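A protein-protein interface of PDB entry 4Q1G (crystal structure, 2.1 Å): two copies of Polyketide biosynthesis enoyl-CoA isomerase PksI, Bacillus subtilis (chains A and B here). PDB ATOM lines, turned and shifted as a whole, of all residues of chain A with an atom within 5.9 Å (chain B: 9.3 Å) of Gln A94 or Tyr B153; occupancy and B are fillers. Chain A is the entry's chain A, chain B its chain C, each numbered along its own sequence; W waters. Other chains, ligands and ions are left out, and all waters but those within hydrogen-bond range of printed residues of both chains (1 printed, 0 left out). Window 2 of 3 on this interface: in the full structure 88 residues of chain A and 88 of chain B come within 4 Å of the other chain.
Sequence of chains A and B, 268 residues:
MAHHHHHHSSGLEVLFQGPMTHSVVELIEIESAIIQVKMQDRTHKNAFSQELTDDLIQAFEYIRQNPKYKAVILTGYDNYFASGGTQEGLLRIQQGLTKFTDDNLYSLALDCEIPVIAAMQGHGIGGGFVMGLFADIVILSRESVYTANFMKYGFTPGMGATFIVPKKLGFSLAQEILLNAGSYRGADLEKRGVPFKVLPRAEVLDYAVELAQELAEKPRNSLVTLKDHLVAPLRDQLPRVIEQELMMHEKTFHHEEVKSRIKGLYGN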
ATOM      1  N   GLY A  85     -12.438  -3.470 -16.783  1.00  0.00           N
ATOM      2  CA  GLY A  85     -12.749  -4.902 -16.704  1.00  0.00           C
ATOM      3  C   GLY A  85     -12.419  -5.448 -15.313  1.00  0.00           C
ATOM      4  O   GLY A  85     -11.391  -5.035 -14.707  1.00  0.00           O
ATOM      5  N   GLN A  87     -10.991  -8.218 -12.613  1.00  0.00           N
ATOM      6  CA  GLN A  87      -9.850  -9.160 -12.669  1.00  0.00           C
ATOM      7  C   GLN A  87     -10.320 -10.520 -13.164  1.00  0.00           C
ATOM      8  O   GLN A  87      -9.695 -11.090 -14.041  1.00  0.00           O
ATOM      9  CB  GLN A  87      -9.155  -9.320 -11.315  1.00  0.00           C
ATOM     10  CG  GLN A  87      -8.639  -8.016 -10.778  1.00  0.00           C
ATOM     11  CD  GLN A  87      -7.749  -7.312 -11.791  1.00  0.00           C
ATOM     12  OE1 GLN A  87      -8.077  -6.206 -12.275  1.00  0.00           O
ATOM     13  NE2 GLN A  87      -6.613  -7.949 -12.134  1.00  0.00           N
ATOM     14  N   GLY A  89     -12.888 -11.181 -15.011  1.00  0.00           N
ATOM     15  CA  GLY A  89     -13.308 -11.096 -16.400  1.00  0.00           C
ATOM     16  C   GLY A  89     -12.119 -11.177 -17.308  1.00  0.00           C
ATOM     17  O   GLY A  89     -12.129 -11.887 -18.340  1.00  0.00           O
ATOM     18  N   LEU A  90     -11.078 -10.454 -16.909  1.00  0.00           N
ATOM     19  CA  LEU A  90      -9.855 -10.362 -17.686  1.00  0.00           C
ATOM     20  C   LEU A  90      -9.118 -11.694 -17.725  1.00  0.00           C
ATOM     21  O   LEU A  90      -8.605 -12.055 -18.773  1.00  0.00           O
ATOM     22  CB  LEU A  90      -8.926  -9.219 -17.186  1.00  0.00           C
ATOM     23  CG  LEU A  90      -9.478  -7.787 -17.363  1.00  0.00           C
ATOM     24  CD1 LEU A  90      -8.703  -6.730 -16.579  1.00  0.00           C
ATOM     25  CD2 LEU A  90      -9.595  -7.413 -18.827  1.00  0.00           C
ATOM     26  N   LEU A  91      -9.066 -12.407 -16.591  1.00  0.00           N
ATOM     27  CA  LEU A  91      -8.453 -13.749 -16.521  1.00  0.00           C
ATOM     28  C   LEU A  91      -9.168 -14.739 -17.448  1.00  0.00           C
ATOM     29  O   LEU A  91      -8.519 -15.532 -18.126  1.00  0.00           O
ATOM     30  CB  LEU A  91      -8.461 -14.302 -15.089  1.00  0.00           C
ATOM     31  CG  LEU A  91      -7.363 -13.772 -14.155  1.00  0.00           C
ATOM     32  CD1 LEU A  91      -7.820 -13.994 -12.716  1.00  0.00           C
ATOM     33  CD2 LEU A  91      -6.002 -14.417 -14.431  1.00  0.00           C
ATOM     34  N   ARG A  92     -10.505 -14.687 -17.450  1.00  0.00           N
ATOM     35  CA  ARG A  92     -11.293 -15.546 -18.310  1.00  0.00           C
ATOM     36  C   ARG A  92     -10.925 -15.351 -19.783  1.00  0.00           C
ATOM     37  O   ARG A  92     -10.872 -16.326 -20.551  1.00  0.00           O
ATOM     38  CB  ARG A  92     -12.751 -15.229 -18.107  1.00  0.00           C
ATOM     39  CG  ARG A  92     -13.249 -15.744 -16.799  1.00  0.00           C
ATOM     40  CD  ARG A  92     -14.235 -16.773 -17.162  1.00  0.00           C
ATOM     41  NE  ARG A  92     -15.459 -16.535 -16.458  1.00  0.00           N
ATOM     42  CZ  ARG A  92     -16.536 -17.265 -16.678  1.00  0.00           C
ATOM     43  NH1 ARG A  92     -16.486 -18.219 -17.605  1.00  0.00           N
ATOM     44  NH2 ARG A  92     -17.660 -17.028 -15.993  1.00  0.00           N
ATOM     45  N   ILE A  93     -10.690 -14.095 -20.167  1.00  0.00           N
ATOM     46  CA  ILE A  93     -10.283 -13.785 -21.531  1.00  0.00           C
ATOM     47  C   ILE A  93      -8.889 -14.388 -21.777  1.00  0.00           C
ATOM     48  O   ILE A  93      -8.744 -15.255 -22.648  1.00  0.00           O
ATOM     49  CB  ILE A  93     -10.358 -12.260 -21.859  1.00  0.00           C
ATOM     50  CG1 ILE A  93     -11.769 -11.682 -21.565  1.00  0.00           C
ATOM     51  CG2 ILE A  93      -9.892 -11.977 -23.299  1.00  0.00           C
ATOM     52  CD1 ILE A  93     -12.823 -12.046 -22.579  1.00  0.00           C
ATOM     53  N   GLN A  94      -7.874 -13.977 -20.998  1.00  0.00           N
ATOM     54  CA  GLN A  94      -6.527 -14.589 -21.125  1.00  0.00           C
ATOM     55  C   GLN A  94      -6.602 -16.099 -21.290  1.00  0.00           C
ATOM     56  O   GLN A  94      -5.881 -16.657 -22.088  1.00  0.00           O
ATOM     57  CB  GLN A  94      -5.584 -14.216 -19.956  1.00  0.00           C
ATOM     58  CG  GLN A  94      -5.177 -12.748 -19.980  1.00  0.00           C
ATOM     59  CD  GLN A  94      -4.521 -12.207 -18.703  1.00  0.00           C
ATOM     60  OE1 GLN A  94      -3.665 -11.318 -18.773  1.00  0.00           O
ATOM     61  NE2 GLN A  94      -4.936 -12.715 -17.539  1.00  0.00           N
ATOM     62  N   GLN A  95      -7.500 -16.749 -20.564  1.00  0.00           N
ATOM     63  CA  GLN A  95      -7.603 -18.201 -20.590  1.00  0.00           C
ATOM     64  C   GLN A  95      -8.523 -18.740 -21.692  1.00  0.00           C
ATOM     65  O   GLN A  95      -8.674 -19.951 -21.845  1.00  0.00           O
ATOM     66  CB  GLN A  95      -8.093 -18.674 -19.231  1.00  0.00           C
ATOM     67  CG  GLN A  95      -6.981 -18.864 -18.221  1.00  0.00           C
ATOM     68  CD  GLN A  95      -6.269 -20.191 -18.418  1.00  0.00           C
ATOM     69  OE1 GLN A  95      -5.393 -20.309 -19.264  1.00  0.00           O
ATOM     70  NE2 GLN A  95      -6.653 -21.195 -17.646  1.00  0.00           N
ATOM     71  N   GLY A  96      -9.140 -17.838 -22.449  1.00  0.00           N
ATOM     72  CA  GLY A  96     -10.120 -18.218 -23.458  1.00  0.00           C
ATOM     73  C   GLY A  96     -11.220 -19.067 -22.862  1.00  0.00           C
ATOM     74  O   GLY A  96     -11.343 -20.241 -23.196  1.00  0.00           O
ATOM     75  N   ILE B 125      -9.372   3.474 -14.716  1.00  0.00           N
ATOM     76  CA  ILE B 125      -8.480   2.421 -15.090  1.00  0.00           C
ATOM     77  C   ILE B 125      -9.103   1.740 -16.275  1.00  0.00           C
ATOM     78  O   ILE B 125     -10.309   1.295 -16.243  1.00  0.00           O
ATOM     79  CB  ILE B 125      -8.326   1.342 -13.968  1.00  0.00           C
ATOM     80  CG1 ILE B 125      -8.120   1.963 -12.558  1.00  0.00           C
ATOM     81  CG2 ILE B 125      -7.333   0.221 -14.388  1.00  0.00           C
ATOM     82  CD1 ILE B 125      -6.758   2.596 -12.414  1.00  0.00           C
ATOM     83  N   GLY B 126      -8.305   1.605 -17.324  1.00  0.00           N
ATOM     84  CA  GLY B 126      -8.694   0.715 -18.440  1.00  0.00           C
ATOM     85  C   GLY B 126      -9.994   1.218 -19.063  1.00  0.00           C
ATOM     86  O   GLY B 126     -10.159   2.434 -19.369  1.00  0.00           O
ATOM     87  N   GLY B 127     -10.927   0.290 -19.239  1.00  0.00           N
ATOM     88  CA  GLY B 127     -12.237   0.649 -19.804  1.00  0.00           C
ATOM     89  C   GLY B 127     -13.030   1.679 -18.999  1.00  0.00           C
ATOM     90  O   GLY B 127     -13.834   2.414 -19.569  1.00  0.00           O
ATOM     91  N   THR B 147      -5.234   5.285 -16.414  1.00  0.00           N
ATOM     92  CA  THR B 147      -4.390   4.423 -17.287  1.00  0.00           C
ATOM     93  C   THR B 147      -5.265   3.753 -18.352  1.00  0.00           C
ATOM     94  O   THR B 147      -6.410   3.367 -18.062  1.00  0.00           O
ATOM     95  CB  THR B 147      -3.604   3.374 -16.465  1.00  0.00           C
ATOM     96  OG1 THR B 147      -2.817   2.572 -17.382  1.00  0.00           O
ATOM     97  CG2 THR B 147      -4.528   2.413 -15.732  1.00  0.00           C
ATOM     98  N   ALA B 148      -4.785   3.689 -19.588  1.00  0.00           N
ATOM     99  CA  ALA B 148      -5.378   2.791 -20.557  1.00  0.00           C
ATOM    100  C   ALA B 148      -4.494   1.538 -20.486  1.00  0.00           C
ATOM    101  O   ALA B 148      -3.585   1.335 -21.353  1.00  0.00           O
ATOM    102  CB  ALA B 148      -5.342   3.429 -21.972  1.00  0.00           C
ATOM    103  N   ASN B 149      -4.756   0.670 -19.512  1.00  0.00           N
ATOM    104  CA  ASN B 149      -3.770  -0.350 -19.172  1.00  0.00           C
ATOM    105  C   ASN B 149      -3.904  -1.684 -19.914  1.00  0.00           C
ATOM    106  O   ASN B 149      -3.250  -2.697 -19.526  1.00  0.00           O
ATOM    107  CB  ASN B 149      -3.707  -0.586 -17.677  1.00  0.00           C
ATOM    108  CG  ASN B 149      -5.009  -1.172 -17.105  1.00  0.00           C
ATOM    109  OD1 ASN B 149      -6.053  -1.154 -17.714  1.00  0.00           O
ATOM    110  ND2 ASN B 149      -4.910  -1.690 -15.921  1.00  0.00           N
ATOM    111  N   PHE B 150      -4.727  -1.691 -20.968  1.00  0.00           N
ATOM    112  CA  PHE B 150      -5.027  -2.931 -21.778  1.00  0.00           C
ATOM    113  C   PHE B 150      -3.774  -3.749 -22.102  1.00  0.00           C
ATOM    114  O   PHE B 150      -3.697  -4.950 -21.794  1.00  0.00           O
ATOM    115  CB  PHE B 150      -5.720  -2.563 -23.071  1.00  0.00           C
ATOM    116  CG  PHE B 150      -6.958  -1.745 -22.845  1.00  0.00           C
ATOM    117  CD1 PHE B 150      -8.160  -2.360 -22.521  1.00  0.00           C
ATOM    118  CD2 PHE B 150      -6.902  -0.314 -22.911  1.00  0.00           C
ATOM    119  CE1 PHE B 150      -9.320  -1.595 -22.298  1.00  0.00           C
ATOM    120  CE2 PHE B 150      -8.053   0.451 -22.695  1.00  0.00           C
ATOM    121  CZ  PHE B 150      -9.262  -0.203 -22.371  1.00  0.00           C
ATOM    122  N   MET B 151      -2.761  -3.070 -22.660  1.00  0.00           N
ATOM    123  CA  MET B 151      -1.493  -3.776 -23.083  1.00  0.00           C
ATOM    124  C   MET B 151      -0.713  -4.387 -21.908  1.00  0.00           C
ATOM    125  O   MET B 151       0.051  -5.349 -22.118  1.00  0.00           O
ATOM    126  CB  MET B 151      -0.569  -2.851 -23.935  1.00  0.00           C
ATOM    127  CG  MET B 151      -1.278  -2.455 -25.229  1.00  0.00           C
ATOM    128  SD  MET B 151      -0.910  -3.724 -26.496  1.00  0.00           S
ATOM    129  CE  MET B 151       0.861  -3.387 -26.868  1.00  0.00           C
ATOM    130  N   LYS B 152      -0.917  -3.866 -20.684  1.00  0.00           N
ATOM    131  CA  LYS B 152      -0.345  -4.499 -19.464  1.00  0.00           C
ATOM    132  C   LYS B 152      -0.833  -5.930 -19.347  1.00  0.00           C
ATOM    133  O   LYS B 152      -0.100  -6.772 -18.918  1.00  0.00           O
ATOM    134  CB  LYS B 152      -0.688  -3.723 -18.159  1.00  0.00           C
ATOM    135  CG  LYS B 152       0.397  -2.779 -17.670  1.00  0.00           C
ATOM    136  CD  LYS B 152       0.649  -2.928 -16.158  1.00  0.00           C
ATOM    137  CE  LYS B 152       1.552  -1.819 -15.586  1.00  0.00           C
ATOM    138  NZ  LYS B 152       2.122  -0.909 -16.627  1.00  0.00           N
ATOM    139  N   TYR B 153      -2.057  -6.227 -19.748  1.00  0.00           N
ATOM    140  CA  TYR B 153      -2.541  -7.614 -19.731  1.00  0.00           C
ATOM    141  C   TYR B 153      -2.107  -8.441 -20.962  1.00  0.00           C
ATOM    142  O   TYR B 153      -2.506  -9.576 -21.111  1.00  0.00           O
ATOM    143  CB  TYR B 153      -4.079  -7.595 -19.640  1.00  0.00           C
ATOM    144  CG  TYR B 153      -4.517  -7.008 -18.298  1.00  0.00           C
ATOM    145  CD1 TYR B 153      -4.473  -7.821 -17.120  1.00  0.00           C
ATOM    146  CD2 TYR B 153      -4.931  -5.667 -18.181  1.00  0.00           C
ATOM    147  CE1 TYR B 153      -4.853  -7.331 -15.876  1.00  0.00           C
ATOM    148  CE2 TYR B 153      -5.315  -5.146 -16.914  1.00  0.00           C
ATOM    149  CZ  TYR B 153      -5.281  -5.967 -15.763  1.00  0.00           C
ATOM    150  OH  TYR B 153      -5.662  -5.502 -14.499  1.00  0.00           O
ATOM    151  N   GLY B 154      -1.326  -7.864 -21.853  1.00  0.00           N
ATOM    152  CA  GLY B 154      -1.028  -8.516 -23.119  1.00  0.00           C
ATOM    153  C   GLY B 154      -2.015  -8.207 -24.218  1.00  0.00           C
ATOM    154  O   GLY B 154      -1.758  -8.568 -25.348  1.00  0.00           O
ATOM    155  N   PHE B 155      -3.106  -7.499 -23.933  1.00  0.00           N
ATOM    156  CA  PHE B 155      -4.119  -7.221 -24.975  1.00  0.00           C
ATOM    157  C   PHE B 155      -3.945  -5.869 -25.650  1.00  0.00           C
ATOM    158  O   PHE B 155      -3.673  -4.881 -24.971  1.00  0.00           O
ATOM    159  CB  PHE B 155      -5.547  -7.207 -24.374  1.00  0.00           C
ATOM    160  CG  PHE B 155      -5.897  -8.449 -23.618  1.00  0.00           C
ATOM    161  CD1 PHE B 155      -5.510  -9.695 -24.095  1.00  0.00           C
ATOM    162  CD2 PHE B 155      -6.639  -8.375 -22.445  1.00  0.00           C
ATOM    163  CE1 PHE B 155      -5.847 -10.865 -23.409  1.00  0.00           C
ATOM    164  CE2 PHE B 155      -6.989  -9.532 -21.750  1.00  0.00           C
ATOM    165  CZ  PHE B 155      -6.603 -10.780 -22.236  1.00  0.00           C
ATOM    166  N   THR B 156      -4.239  -5.815 -26.961  1.00  0.00           N
ATOM    167  CA  THR B 156      -4.394  -4.549 -27.654  1.00  0.00           C
ATOM    168  C   THR B 156      -5.678  -3.843 -27.138  1.00  0.00           C
ATOM    169  O   THR B 156      -6.586  -4.484 -26.594  1.00  0.00           O
ATOM    170  CB  THR B 156      -4.443  -4.734 -29.162  1.00  0.00           C
ATOM    171  OG1 THR B 156      -5.421  -5.750 -29.440  1.00  0.00           O
ATOM    172  CG2 THR B 156      -2.993  -5.176 -29.693  1.00  0.00           C
ATOM    173  N   PRO B 157      -5.728  -2.511 -27.241  1.00  0.00           N
ATOM    174  CA  PRO B 157      -6.780  -1.812 -26.487  1.00  0.00           C
ATOM    175  C   PRO B 157      -8.161  -2.033 -27.092  1.00  0.00           C
ATOM    176  O   PRO B 157      -8.281  -2.271 -28.272  1.00  0.00           O
ATOM    177  CB  PRO B 157      -6.358  -0.350 -26.559  1.00  0.00           C
ATOM    178  CG  PRO B 157      -4.862  -0.439 -26.730  1.00  0.00           C
ATOM    179  CD  PRO B 157      -4.708  -1.574 -27.725  1.00  0.00           C
ATOM    180  N   LEU B 178      -1.244   4.411 -24.999  1.00  0.00           N
ATOM    181  CA  LEU B 178      -1.771   3.184 -25.530  1.00  0.00           C
ATOM    182  C   LEU B 178      -0.703   2.100 -25.700  1.00  0.00           C
ATOM    183  O   LEU B 178      -0.963   0.995 -25.223  1.00  0.00           O
ATOM    184  CB  LEU B 178      -2.588   3.418 -26.831  1.00  0.00           C
ATOM    185  CG  LEU B 178      -3.800   4.344 -26.679  1.00  0.00           C
ATOM    186  CD1 LEU B 178      -4.282   4.716 -28.090  1.00  0.00           C
ATOM    187  CD2 LEU B 178      -4.903   3.592 -25.948  1.00  0.00           C
ATOM    188  N   LEU B 179       0.512   2.429 -26.239  1.00  0.00           N
ATOM    189  CA  LEU B 179       1.590   1.439 -26.444  1.00  0.00           C
ATOM    190  C   LEU B 179       2.117   0.953 -25.104  1.00  0.00           C
ATOM    191  O   LEU B 179       2.340  -0.242 -24.936  1.00  0.00           O
ATOM    192  CB  LEU B 179       2.759   1.997 -27.303  1.00  0.00           C
ATOM    193  CG  LEU B 179       2.446   2.195 -28.784  1.00  0.00           C
ATOM    194  CD1 LEU B 179       3.516   3.036 -29.499  1.00  0.00           C
ATOM    195  CD2 LEU B 179       2.326   0.828 -29.504  1.00  0.00           C
ATOM    196  N   ASN B 180       2.253   1.879 -24.151  1.00  0.00           N
ATOM    197  CA  ASN B 180       2.882   1.571 -22.912  1.00  0.00           C
ATOM    198  C   ASN B 180       1.928   1.184 -21.784  1.00  0.00           C
ATOM    199  O   ASN B 180       2.363   0.495 -20.842  1.00  0.00           O
ATOM    200  CB  ASN B 180       3.949   2.613 -22.519  1.00  0.00           C
ATOM    201  CG  ASN B 180       4.991   2.058 -21.551  1.00  0.00           C
ATOM    202  OD1 ASN B 180       5.427   0.899 -21.610  1.00  0.00           O
ATOM    203  ND2 ASN B 180       5.272   2.839 -20.547  1.00  0.00           N
ATOM    204  N   ALA B 181       0.655   1.599 -21.887  1.00  0.00           N
ATOM    205  CA  ALA B 181      -0.338   1.249 -20.892  1.00  0.00           C
ATOM    206  C   ALA B 181       0.142   1.695 -19.562  1.00  0.00           C
ATOM    207  O   ALA B 181      -0.160   1.024 -18.550  1.00  0.00           O
ATOM    208  CB  ALA B 181      -0.595  -0.267 -20.861  1.00  0.00           C
ATOM    209  N   HIS B 249      -7.499  -8.211 -31.616  1.00  0.00           N
ATOM    210  CA  HIS B 249      -7.577  -9.426 -30.847  1.00  0.00           C
ATOM    211  C   HIS B 249      -7.761 -10.426 -31.912  1.00  0.00           C
ATOM    212  O   HIS B 249      -8.190 -10.084 -32.974  1.00  0.00           O
ATOM    213  CB  HIS B 249      -8.783  -9.429 -29.920  1.00  0.00           C
ATOM    214  CG  HIS B 249      -8.861  -8.238 -29.016  1.00  0.00           C
ATOM    215  ND1 HIS B 249      -9.991  -7.591 -28.789  1.00  0.00           N
ATOM    216  CD2 HIS B 249      -7.900  -7.581 -28.299  1.00  0.00           C
ATOM    217  CE1 HIS B 249      -9.774  -6.572 -27.965  1.00  0.00           C
ATOM    218  NE2 HIS B 249      -8.500  -6.576 -27.654  1.00  0.00           N
HETATM  219  O   HOH W   1     -10.591  -2.377 -18.688  1.00  0.00           O
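The backbone NH (N) of Phe B155 lies within hydrogen-bond range of the backbone carbonyl oxygen (O) of Phe B150 (3.4 Å).
No position is printed for both chains.
Of the 5 pairs that touch across the chains among the printed residues, none has its exchanged pair printed and touching as well.
Of the printed residues of chain B, Gln A87 touches Tyr B153 (3.4 Å).
Printed residues of chain B within 4 Å of Leu A90: Tyr B153 (3.6 Å).
Printed residues of chain B within 4 Å of Ile A93: Phe B155.
Tyr B153 touches just these residues of chain A: Gln A87, Leu A90 and Gln A94.
Printed residues of chain A within 4 Å of Phe B155: Ile A93 (3.7 Å) and Gln A94 (3.3 Å).
The nearest residue of chain B that does not touch Gln A94 is Gly B154 (5.2 Å).
The nearest printed residue of chain B that does not touch Ile A93 is His B249 (6.9 Å).
Among the printed residues, merely in contact across the chains: Gln A94 with Phe B155 (3.3 Å), Leu A90 with Tyr B153 (3.6 Å) and Ile A93 with Phe B155 (3.7 Å).
Along chain A the printed residues that touch a printed residue of chain B span positions 87 to 94.
The side-chain amide oxygen (OE1) of Gln A87 sits at hydrogen-bond distance from the side-chain hydroxyl (OH) of Tyr B153, 3.4 Å away.
The backbone carbonyl oxygen (O) of Tyr B153 sits close to the side-chain amide oxygen (OE1) of Gln A94 (3.1 Å).
Water W1 lies within hydrogen-bond range of N of Gly B127 and N of Gly A85.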
